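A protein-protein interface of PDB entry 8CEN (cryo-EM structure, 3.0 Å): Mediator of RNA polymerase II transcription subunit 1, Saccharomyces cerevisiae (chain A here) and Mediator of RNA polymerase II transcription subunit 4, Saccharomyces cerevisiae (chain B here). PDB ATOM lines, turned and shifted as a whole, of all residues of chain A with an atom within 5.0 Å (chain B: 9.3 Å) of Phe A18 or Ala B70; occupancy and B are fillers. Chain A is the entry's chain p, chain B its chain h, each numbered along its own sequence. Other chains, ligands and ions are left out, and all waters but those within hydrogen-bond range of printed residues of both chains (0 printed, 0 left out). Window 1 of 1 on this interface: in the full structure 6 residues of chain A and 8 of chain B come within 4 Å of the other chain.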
ATOM      1  N   MET A  14     -11.614  22.873 -19.358  1.00  0.00           N
ATOM      2  CA  MET A  14     -12.150  21.737 -18.610  1.00  0.00           C
ATOM      3  C   MET A  14     -13.483  22.080 -17.950  1.00  0.00           C
ATOM      4  O   MET A  14     -14.354  21.209 -17.836  1.00  0.00           O
ATOM      5  CB  MET A  14     -11.150  21.204 -17.578  1.00  0.00           C
ATOM      6  CG  MET A  14     -10.878  22.047 -16.346  1.00  0.00           C
ATOM      7  SD  MET A  14      -9.436  21.375 -15.491  1.00  0.00           S
ATOM      8  CE  MET A  14      -8.945  22.738 -14.445  1.00  0.00           C
ATOM      9  N   ILE A  15     -13.686  23.336 -17.528  1.00  0.00           N
ATOM     10  CA  ILE A  15     -15.018  23.660 -17.020  1.00  0.00           C
ATOM     11  C   ILE A  15     -16.024  23.717 -18.169  1.00  0.00           C
ATOM     12  O   ILE A  15     -17.199  23.376 -17.985  1.00  0.00           O
ATOM     13  CB  ILE A  15     -15.024  24.954 -16.179  1.00  0.00           C
ATOM     14  CG1 ILE A  15     -14.660  26.179 -17.014  1.00  0.00           C
ATOM     15  CG2 ILE A  15     -14.080  24.808 -14.992  1.00  0.00           C
ATOM     16  CD1 ILE A  15     -14.883  27.501 -16.312  1.00  0.00           C
ATOM     17  N   GLU A  16     -15.579  24.093 -19.377  1.00  0.00           N
ATOM     18  CA  GLU A  16     -16.442  24.012 -20.553  1.00  0.00           C
ATOM     19  C   GLU A  16     -16.807  22.567 -20.876  1.00  0.00           C
ATOM     20  O   GLU A  16     -17.944  22.276 -21.259  1.00  0.00           O
ATOM     21  CB  GLU A  16     -15.753  24.679 -21.745  1.00  0.00           C
ATOM     22  CG  GLU A  16     -16.463  24.522 -23.087  1.00  0.00           C
ATOM     23  CD  GLU A  16     -17.802  25.229 -23.146  1.00  0.00           C
ATOM     24  OE1 GLU A  16     -17.977  26.251 -22.449  1.00  0.00           O
ATOM     25  OE2 GLU A  16     -18.681  24.767 -23.904  1.00  0.00           O
ATOM     26  N   LEU A  17     -15.853  21.650 -20.720  1.00  0.00           N
ATOM     27  CA  LEU A  17     -16.110  20.240 -20.996  1.00  0.00           C
ATOM     28  C   LEU A  17     -17.054  19.632 -19.958  1.00  0.00           C
ATOM     29  O   LEU A  17     -17.931  18.824 -20.300  1.00  0.00           O
ATOM     30  CB  LEU A  17     -14.780  19.490 -21.047  1.00  0.00           C
ATOM     31  CG  LEU A  17     -14.766  18.005 -21.389  1.00  0.00           C
ATOM     32  CD1 LEU A  17     -15.299  17.768 -22.795  1.00  0.00           C
ATOM     33  CD2 LEU A  17     -13.364  17.434 -21.236  1.00  0.00           C
ATOM     34  N   PHE A  18     -16.886  20.011 -18.684  1.00  0.00           N
ATOM     35  CA  PHE A  18     -17.827  19.595 -17.642  1.00  0.00           C
ATOM     36  C   PHE A  18     -19.218  20.162 -17.900  1.00  0.00           C
ATOM     37  O   PHE A  18     -20.227  19.498 -17.635  1.00  0.00           O
ATOM     38  CB  PHE A  18     -17.334  20.025 -16.253  1.00  0.00           C
ATOM     39  CG  PHE A  18     -16.044  19.366 -15.794  1.00  0.00           C
ATOM     40  CD1 PHE A  18     -15.426  18.361 -16.530  1.00  0.00           C
ATOM     41  CD2 PHE A  18     -15.449  19.773 -14.609  1.00  0.00           C
ATOM     42  CE1 PHE A  18     -14.249  17.780 -16.093  1.00  0.00           C
ATOM     43  CE2 PHE A  18     -14.271  19.195 -14.167  1.00  0.00           C
ATOM     44  CZ  PHE A  18     -13.672  18.198 -14.910  1.00  0.00           C
ATOM     45  N   LYS A  19     -19.286  21.401 -18.396  1.00  0.00           N
ATOM     46  CA  LYS A  19     -20.554  21.983 -18.822  1.00  0.00           C
ATOM     47  C   LYS A  19     -21.175  21.194 -19.969  1.00  0.00           C
ATOM     48  O   LYS A  19     -22.389  20.961 -19.991  1.00  0.00           O
ATOM     49  CB  LYS A  19     -20.325  23.432 -19.251  1.00  0.00           C
ATOM     50  CG  LYS A  19     -21.584  24.186 -19.588  1.00  0.00           C
ATOM     51  CD  LYS A  19     -21.281  25.608 -20.021  1.00  0.00           C
ATOM     52  CE  LYS A  19     -20.832  26.452 -18.864  1.00  0.00           C
ATOM     53  NZ  LYS A  19     -21.965  26.631 -17.919  1.00  0.00           N
ATOM     54  N   ASP A  20     -20.351  20.785 -20.936  1.00  0.00           N
ATOM     55  CA  ASP A  20     -20.854  20.122 -22.133  1.00  0.00           C
ATOM     56  C   ASP A  20     -21.331  18.704 -21.849  1.00  0.00           C
ATOM     57  O   ASP A  20     -22.251  18.222 -22.520  1.00  0.00           O
ATOM     58  CB  ASP A  20     -19.771  20.102 -23.214  1.00  0.00           C
ATOM     59  CG  ASP A  20     -20.347  20.012 -24.615  1.00  0.00           C
ATOM     60  OD1 ASP A  20     -21.588  20.003 -24.751  1.00  0.00           O
ATOM     61  OD2 ASP A  20     -19.557  19.941 -25.580  1.00  0.00           O
ATOM     62  N   TYR A  21     -20.724  18.017 -20.881  1.00  0.00           N
ATOM     63  CA  TYR A  21     -21.120  16.629 -20.658  1.00  0.00           C
ATOM     64  C   TYR A  21     -22.480  16.495 -19.980  1.00  0.00           C
ATOM     65  O   TYR A  21     -23.439  16.045 -20.616  1.00  0.00           O
ATOM     66  CB  TYR A  21     -20.050  15.895 -19.843  1.00  0.00           C
ATOM     67  CG  TYR A  21     -20.538  14.618 -19.188  1.00  0.00           C
ATOM     68  CD1 TYR A  21     -20.930  13.521 -19.947  1.00  0.00           C
ATOM     69  CD2 TYR A  21     -20.581  14.505 -17.801  1.00  0.00           C
ATOM     70  CE1 TYR A  21     -21.373  12.359 -19.344  1.00  0.00           C
ATOM     71  CE2 TYR A  21     -21.022  13.349 -17.191  1.00  0.00           C
ATOM     72  CZ  TYR A  21     -21.413  12.280 -17.966  1.00  0.00           C
ATOM     73  OH  TYR A  21     -21.850  11.127 -17.360  1.00  0.00           O
ATOM     74  N   LYS A  22     -22.590  16.900 -18.714  1.00  0.00           N
ATOM     75  CA  LYS A  22     -23.846  16.733 -17.993  1.00  0.00           C
ATOM     76  C   LYS A  22     -23.868  17.653 -16.781  1.00  0.00           C
ATOM     77  O   LYS A  22     -23.345  17.292 -15.718  1.00  0.00           O
ATOM     78  CB  LYS A  22     -24.045  15.273 -17.570  1.00  0.00           C
ATOM     79  CG  LYS A  22     -25.361  14.990 -16.866  1.00  0.00           C
ATOM     80  CD  LYS A  22     -25.523  13.506 -16.586  1.00  0.00           C
ATOM     81  CE  LYS A  22     -26.765  13.240 -15.756  1.00  0.00           C
ATOM     82  NZ  LYS A  22     -28.002  13.577 -16.515  1.00  0.00           N
ATOM     83  N   PRO A  23     -24.437  18.849 -16.893  1.00  0.00           N
ATOM     84  CA  PRO A  23     -24.510  19.775 -15.756  1.00  0.00           C
ATOM     85  C   PRO A  23     -25.684  19.514 -14.810  1.00  0.00           C
ATOM     86  O   PRO A  23     -26.499  20.398 -14.540  1.00  0.00           O
ATOM     87  CB  PRO A  23     -24.615  21.142 -16.438  1.00  0.00           C
ATOM     88  CG  PRO A  23     -25.218  20.872 -17.763  1.00  0.00           C
ATOM     89  CD  PRO A  23     -24.918  19.455 -18.146  1.00  0.00           C
ATOM     90  N   TYR B  49     -13.443   6.545  -9.848  1.00  0.00           N
ATOM     91  CA  TYR B  49     -13.920   7.927  -9.813  1.00  0.00           C
ATOM     92  C   TYR B  49     -13.050   8.778  -8.888  1.00  0.00           C
ATOM     93  O   TYR B  49     -12.629   9.888  -9.249  1.00  0.00           O
ATOM     94  CB  TYR B  49     -15.388   7.959  -9.376  1.00  0.00           C
ATOM     95  CG  TYR B  49     -16.077   9.294  -9.572  1.00  0.00           C
ATOM     96  CD1 TYR B  49     -16.071  10.260  -8.572  1.00  0.00           C
ATOM     97  CD2 TYR B  49     -16.738   9.585 -10.759  1.00  0.00           C
ATOM     98  CE1 TYR B  49     -16.703  11.479  -8.751  1.00  0.00           C
ATOM     99  CE2 TYR B  49     -17.373  10.800 -10.947  1.00  0.00           C
ATOM    100  CZ  TYR B  49     -17.352  11.742  -9.939  1.00  0.00           C
ATOM    101  OH  TYR B  49     -17.981  12.953 -10.122  1.00  0.00           O
ATOM    102  N   THR B  52      -9.611   9.240 -10.581  1.00  0.00           N
ATOM    103  CA  THR B  52      -9.625  10.260 -11.625  1.00  0.00           C
ATOM    104  C   THR B  52      -9.675  11.664 -11.034  1.00  0.00           C
ATOM    105  O   THR B  52      -8.945  12.554 -11.485  1.00  0.00           O
ATOM    106  CB  THR B  52     -10.799  10.039 -12.580  1.00  0.00           C
ATOM    107  OG1 THR B  52     -12.000   9.819 -11.831  1.00  0.00           O
ATOM    108  CG2 THR B  52     -10.531   8.856 -13.504  1.00  0.00           C
ATOM    109  N   LEU B  53     -10.507  11.880 -10.006  1.00  0.00           N
ATOM    110  CA  LEU B  53     -10.556  13.218  -9.413  1.00  0.00           C
ATOM    111  C   LEU B  53      -9.268  13.552  -8.662  1.00  0.00           C
ATOM    112  O   LEU B  53      -8.831  14.708  -8.677  1.00  0.00           O
ATOM    113  CB  LEU B  53     -11.784  13.372  -8.508  1.00  0.00           C
ATOM    114  CG  LEU B  53     -12.035  12.554  -7.236  1.00  0.00           C
ATOM    115  CD1 LEU B  53     -11.387  13.162  -5.991  1.00  0.00           C
ATOM    116  CD2 LEU B  53     -13.531  12.368  -7.017  1.00  0.00           C
ATOM    117  N   LYS B  55      -6.169  12.384  -9.400  1.00  0.00           N
ATOM    118  CA  LYS B  55      -5.145  12.704 -10.389  1.00  0.00           C
ATOM    119  C   LYS B  55      -5.426  14.033 -11.080  1.00  0.00           C
ATOM    120  O   LYS B  55      -4.484  14.752 -11.428  1.00  0.00           O
ATOM    121  CB  LYS B  55      -5.016  11.573 -11.409  1.00  0.00           C
ATOM    122  CG  LYS B  55      -3.940  10.539 -11.073  1.00  0.00           C
ATOM    123  CD  LYS B  55      -4.351   9.615  -9.938  1.00  0.00           C
ATOM    124  CE  LYS B  55      -3.308   8.535  -9.699  1.00  0.00           C
ATOM    125  NZ  LYS B  55      -3.636   7.697  -8.512  1.00  0.00           N
ATOM    126  N   LEU B  56      -6.702  14.400 -11.252  1.00  0.00           N
ATOM    127  CA  LEU B  56      -7.020  15.699 -11.839  1.00  0.00           C
ATOM    128  C   LEU B  56      -6.642  16.841 -10.898  1.00  0.00           C
ATOM    129  O   LEU B  56      -6.097  17.862 -11.340  1.00  0.00           O
ATOM    130  CB  LEU B  56      -8.507  15.747 -12.212  1.00  0.00           C
ATOM    131  CG  LEU B  56      -9.112  16.898 -13.030  1.00  0.00           C
ATOM    132  CD1 LEU B  56     -10.306  16.378 -13.813  1.00  0.00           C
ATOM    133  CD2 LEU B  56      -9.556  18.078 -12.170  1.00  0.00           C
ATOM    134  N   VAL B  57      -6.918  16.690  -9.597  1.00  0.00           N
ATOM    135  CA  VAL B  57      -6.547  17.749  -8.662  1.00  0.00           C
ATOM    136  C   VAL B  57      -5.031  17.795  -8.482  1.00  0.00           C
ATOM    137  O   VAL B  57      -4.458  18.878  -8.310  1.00  0.00           O
ATOM    138  CB  VAL B  57      -7.307  17.617  -7.321  1.00  0.00           C
ATOM    139  CG1 VAL B  57      -6.902  16.391  -6.536  1.00  0.00           C
ATOM    140  CG2 VAL B  57      -7.114  18.860  -6.472  1.00  0.00           C
ATOM    141  N   SER B  59      -2.942  17.145 -10.974  1.00  0.00           N
ATOM    142  CA  SER B  59      -2.494  17.807 -12.196  1.00  0.00           C
ATOM    143  C   SER B  59      -2.705  19.315 -12.129  1.00  0.00           C
ATOM    144  O   SER B  59      -1.823  20.087 -12.526  1.00  0.00           O
ATOM    145  CB  SER B  59      -3.217  17.217 -13.407  1.00  0.00           C
ATOM    146  OG  SER B  59      -4.572  17.630 -13.443  1.00  0.00           O
ATOM    147  N   VAL B  60      -3.858  19.761 -11.623  1.00  0.00           N
ATOM    148  CA  VAL B  60      -4.088  21.203 -11.550  1.00  0.00           C
ATOM    149  C   VAL B  60      -3.268  21.839 -10.426  1.00  0.00           C
ATOM    150  O   VAL B  60      -2.921  23.024 -10.515  1.00  0.00           O
ATOM    151  CB  VAL B  60      -5.594  21.518 -11.418  1.00  0.00           C
ATOM    152  CG1 VAL B  60      -6.152  21.068 -10.084  1.00  0.00           C
ATOM    153  CG2 VAL B  60      -5.893  22.995 -11.683  1.00  0.00           C
ATOM    154  N   PRO B  65      -2.718  20.626 -16.154  1.00  0.00           N
ATOM    155  CA  PRO B  65      -3.966  19.863 -16.249  1.00  0.00           C
ATOM    156  C   PRO B  65      -4.068  19.126 -17.576  1.00  0.00           C
ATOM    157  O   PRO B  65      -3.420  19.469 -18.568  1.00  0.00           O
ATOM    158  CB  PRO B  65      -5.059  20.934 -16.128  1.00  0.00           C
ATOM    159  CG  PRO B  65      -4.357  22.176 -15.652  1.00  0.00           C
ATOM    160  CD  PRO B  65      -2.971  22.076 -16.196  1.00  0.00           C
ATOM    161  N   ASN B  66      -4.905  18.090 -17.581  1.00  0.00           N
ATOM    162  CA  ASN B  66      -5.101  17.252 -18.754  1.00  0.00           C
ATOM    163  C   ASN B  66      -6.584  17.150 -19.078  1.00  0.00           C
ATOM    164  O   ASN B  66      -7.436  17.180 -18.187  1.00  0.00           O
ATOM    165  CB  ASN B  66      -4.513  15.850 -18.547  1.00  0.00           C
ATOM    166  CG  ASN B  66      -3.029  15.879 -18.237  1.00  0.00           C
ATOM    167  OD1 ASN B  66      -2.600  15.472 -17.156  1.00  0.00           O
ATOM    168  ND2 ASN B  66      -2.236  16.362 -19.186  1.00  0.00           N
ATOM    169  N   LEU B  67      -6.883  17.031 -20.373  1.00  0.00           N
ATOM    170  CA  LEU B  67      -8.254  16.881 -20.842  1.00  0.00           C
ATOM    171  C   LEU B  67      -8.630  15.437 -21.145  1.00  0.00           C
ATOM    172  O   LEU B  67      -9.819  15.103 -21.102  1.00  0.00           O
ATOM    173  CB  LEU B  67      -8.485  17.733 -22.096  1.00  0.00           C
ATOM    174  CG  LEU B  67      -8.084  19.207 -22.008  1.00  0.00           C
ATOM    175  CD1 LEU B  67      -8.382  19.922 -23.317  1.00  0.00           C
ATOM    176  CD2 LEU B  67      -8.792  19.891 -20.847  1.00  0.00           C
ATOM    177  N   ASP B  68      -7.650  14.579 -21.446  1.00  0.00           N
ATOM    178  CA  ASP B  68      -7.938  13.160 -21.631  1.00  0.00           C
ATOM    179  C   ASP B  68      -8.427  12.526 -20.335  1.00  0.00           C
ATOM    180  O   ASP B  68      -9.369  11.725 -20.341  1.00  0.00           O
ATOM    181  CB  ASP B  68      -6.696  12.433 -22.149  1.00  0.00           C
ATOM    182  CG  ASP B  68      -6.258  12.927 -23.513  1.00  0.00           C
ATOM    183  OD1 ASP B  68      -7.131  13.339 -24.305  1.00  0.00           O
ATOM    184  OD2 ASP B  68      -5.042  12.900 -23.794  1.00  0.00           O
ATOM    185  N   ILE B  69      -7.813  12.889 -19.206  1.00  0.00           N
ATOM    186  CA  ILE B  69      -8.281  12.370 -17.929  1.00  0.00           C
ATOM    187  C   ILE B  69      -9.602  13.020 -17.524  1.00  0.00           C
ATOM    188  O   ILE B  69     -10.396  12.402 -16.808  1.00  0.00           O
ATOM    189  CB  ILE B  69      -7.182  12.533 -16.857  1.00  0.00           C
ATOM    190  CG1 ILE B  69      -7.498  11.681 -15.626  1.00  0.00           C
ATOM    191  CG2 ILE B  69      -6.989  13.994 -16.468  1.00  0.00           C
ATOM    192  CD1 ILE B  69      -6.287  11.353 -14.805  1.00  0.00           C
ATOM    193  N   ALA B  70      -9.888  14.234 -18.007  1.00  0.00           N
ATOM    194  CA  ALA B  70     -11.211  14.817 -17.802  1.00  0.00           C
ATOM    195  C   ALA B  70     -12.276  14.043 -18.572  1.00  0.00           C
ATOM    196  O   ALA B  70     -13.376  13.805 -18.058  1.00  0.00           O
ATOM    197  CB  ALA B  70     -11.209  16.288 -18.215  1.00  0.00           C
ATOM    198  N   LYS B  71     -11.959  13.634 -19.803  1.00  0.00           N
ATOM    199  CA  LYS B  71     -12.869  12.790 -20.574  1.00  0.00           C
ATOM    200  C   LYS B  71     -13.041  11.422 -19.917  1.00  0.00           C
ATOM    201  O   LYS B  71     -14.141  10.852 -19.925  1.00  0.00           O
ATOM    202  CB  LYS B  71     -12.351  12.649 -22.008  1.00  0.00           C
ATOM    203  CG  LYS B  71     -13.116  11.658 -22.874  1.00  0.00           C
ATOM    204  CD  LYS B  71     -12.494  11.525 -24.257  1.00  0.00           C
ATOM    205  CE  LYS B  71     -11.002  11.240 -24.176  1.00  0.00           C
ATOM    206  NZ  LYS B  71     -10.721   9.963 -23.463  1.00  0.00           N
ATOM    207  N   ASP B  72     -11.961  10.880 -19.346  1.00  0.00           N
ATOM    208  CA  ASP B  72     -12.058   9.616 -18.619  1.00  0.00           C
ATOM    209  C   ASP B  72     -12.942   9.751 -17.382  1.00  0.00           C
ATOM    210  O   ASP B  72     -13.738   8.855 -17.081  1.00  0.00           O
ATOM    211  CB  ASP B  72     -10.664   9.123 -18.234  1.00  0.00           C
ATOM    212  CG  ASP B  72     -10.652   7.656 -17.849  1.00  0.00           C
ATOM    213  OD1 ASP B  72     -11.014   7.338 -16.696  1.00  0.00           O
ATOM    214  OD2 ASP B  72     -10.284   6.820 -18.701  1.00  0.00           O
ATOM    215  N   LEU B  73     -12.815  10.865 -16.654  1.00  0.00           N
ATOM    216  CA  LEU B  73     -13.693  11.135 -15.519  1.00  0.00           C
ATOM    217  C   LEU B  73     -15.139  11.325 -15.964  1.00  0.00           C
ATOM    218  O   LEU B  73     -16.067  10.984 -15.222  1.00  0.00           O
ATOM    219  CB  LEU B  73     -13.195  12.366 -14.755  1.00  0.00           C
ATOM    220  CG  LEU B  73     -13.896  12.784 -13.458  1.00  0.00           C
ATOM    221  CD1 LEU B  73     -12.869  13.175 -12.409  1.00  0.00           C
ATOM    222  CD2 LEU B  73     -14.861  13.939 -13.696  1.00  0.00           C
ATOM    223  N   ILE B  74     -15.339  11.882 -17.160  1.00  0.00           N
ATOM    224  CA  ILE B  74     -16.671  11.962 -17.756  1.00  0.00           C
ATOM    225  C   ILE B  74     -17.232  10.567 -18.004  1.00  0.00           C
ATOM    226  O   ILE B  74     -18.416  10.303 -17.750  1.00  0.00           O
ATOM    227  CB  ILE B  74     -16.609  12.803 -19.047  1.00  0.00           C
ATOM    228  CG1 ILE B  74     -16.725  14.290 -18.723  1.00  0.00           C
ATOM    229  CG2 ILE B  74     -17.630  12.352 -20.089  1.00  0.00           C
ATOM    230  CD1 ILE B  74     -16.458  15.161 -19.903  1.00  0.00           C
ATOM    231  N   ARG B  75     -16.388   9.651 -18.488  1.00  0.00           N
ATOM    232  CA  ARG B  75     -16.823   8.275 -18.717  1.00  0.00           C
ATOM    233  C   ARG B  75     -17.206   7.580 -17.415  1.00  0.00           C
ATOM    234  O   ARG B  75     -18.117   6.744 -17.401  1.00  0.00           O
ATOM    235  CB  ARG B  75     -15.725   7.493 -19.437  1.00  0.00           C
ATOM    236  CG  ARG B  75     -16.159   6.133 -19.958  1.00  0.00           C
ATOM    237  CD  ARG B  75     -16.860   6.255 -21.300  1.00  0.00           C
ATOM    238  NE  ARG B  75     -15.980   6.806 -22.324  1.00  0.00           N
ATOM    239  CZ  ARG B  75     -15.118   6.093 -23.036  1.00  0.00           C
ATOM    240  NH1 ARG B  75     -14.990   4.788 -22.862  1.00  0.00           N
ATOM    241  NH2 ARG B  75     -14.365   6.704 -23.945  1.00  0.00           N
ATOM    242  N   THR B  76     -16.536   7.919 -16.314  1.00  0.00           N
ATOM    243  CA  THR B  76     -16.828   7.317 -15.020  1.00  0.00           C
ATOM    244  C   THR B  76     -18.038   7.928 -14.323  1.00  0.00           C
ATOM    245  O   THR B  76     -18.532   7.338 -13.356  1.00  0.00           O
ATOM    246  CB  THR B  76     -15.611   7.433 -14.099  1.00  0.00           C
ATOM    247  OG1 THR B  76     -15.312   8.813 -13.859  1.00  0.00           O
ATOM    248  CG2 THR B  76     -14.404   6.734 -14.705  1.00  0.00           C
ATOM    249  N   ASP B  77     -18.522   9.085 -14.776  1.00  0.00           N
ATOM    250  CA  ASP B  77     -19.588   9.782 -14.061  1.00  0.00           C
ATOM    251  C   ASP B  77     -20.943   9.109 -14.274  1.00  0.00           C
ATOM    252  O   ASP B  77     -21.729   8.965 -13.328  1.00  0.00           O
ATOM    253  CB  ASP B  77     -19.635  11.247 -14.503  1.00  0.00           C
ATOM    254  CG  ASP B  77     -20.416  12.128 -13.542  1.00  0.00           C
ATOM    255  OD1 ASP B  77     -20.883  11.618 -12.502  1.00  0.00           O
ATOM    256  OD2 ASP B  77     -20.561  13.334 -13.829  1.00  0.00           O
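The side-chain hydroxyl of Ser B59 sits at hydrogen-bond distance from the backbone carbonyl oxygen of Leu B56 (2.6 Å).
Of the printed residues of chain A, Ala B70 touches Leu A17 and Phe A18.
Of the printed residues of chain B, Leu A17 touches Ala B70 (3.9 Å) and Ile B74 (3.6 Å).
Printed residues of chain A within 4 Å of Leu B56: Phe A18 (3.98 Å).
Of the printed residues of chain A, Ile B74 touches Leu A17 (3.6 Å) and Tyr A21 (3.5 Å).
Printed residues of chain B within 4 Å of Tyr A21: Ile B74 (3.5 Å) and Asp B77 (3.4 Å).
Of the printed residues of chain A, Asp B77 touches Tyr A21 (3.4 Å).
The nearest printed residue of chain B that does not touch Phe A18 is Leu B73 (4.6 Å).
The nearest printed residue of chain A that does not touch Ala B70 is Met A14 (5.0 Å).
The nearest printed residue of chain B that does not touch Tyr A21 is Arg B75 (5.7 Å).
Along chain B the printed residues that touch a printed residue of chain A span positions 56 to 77.
Printed residues of chain A that touch a printed residue of chain B: Leu A17, Phe A18 and Tyr A21.
Along chain A the printed residues that touch a printed residue of chain B span positions 17 to 21.
Among the printed residues, pairs that only touch across the chains: Leu A17 with Ala B70, Leu A17 with Ile B74, Phe A18 with Leu B56, Phe A18 with Ala B70, Tyr A21 with Ile B74 and Tyr A21 with Asp B77.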
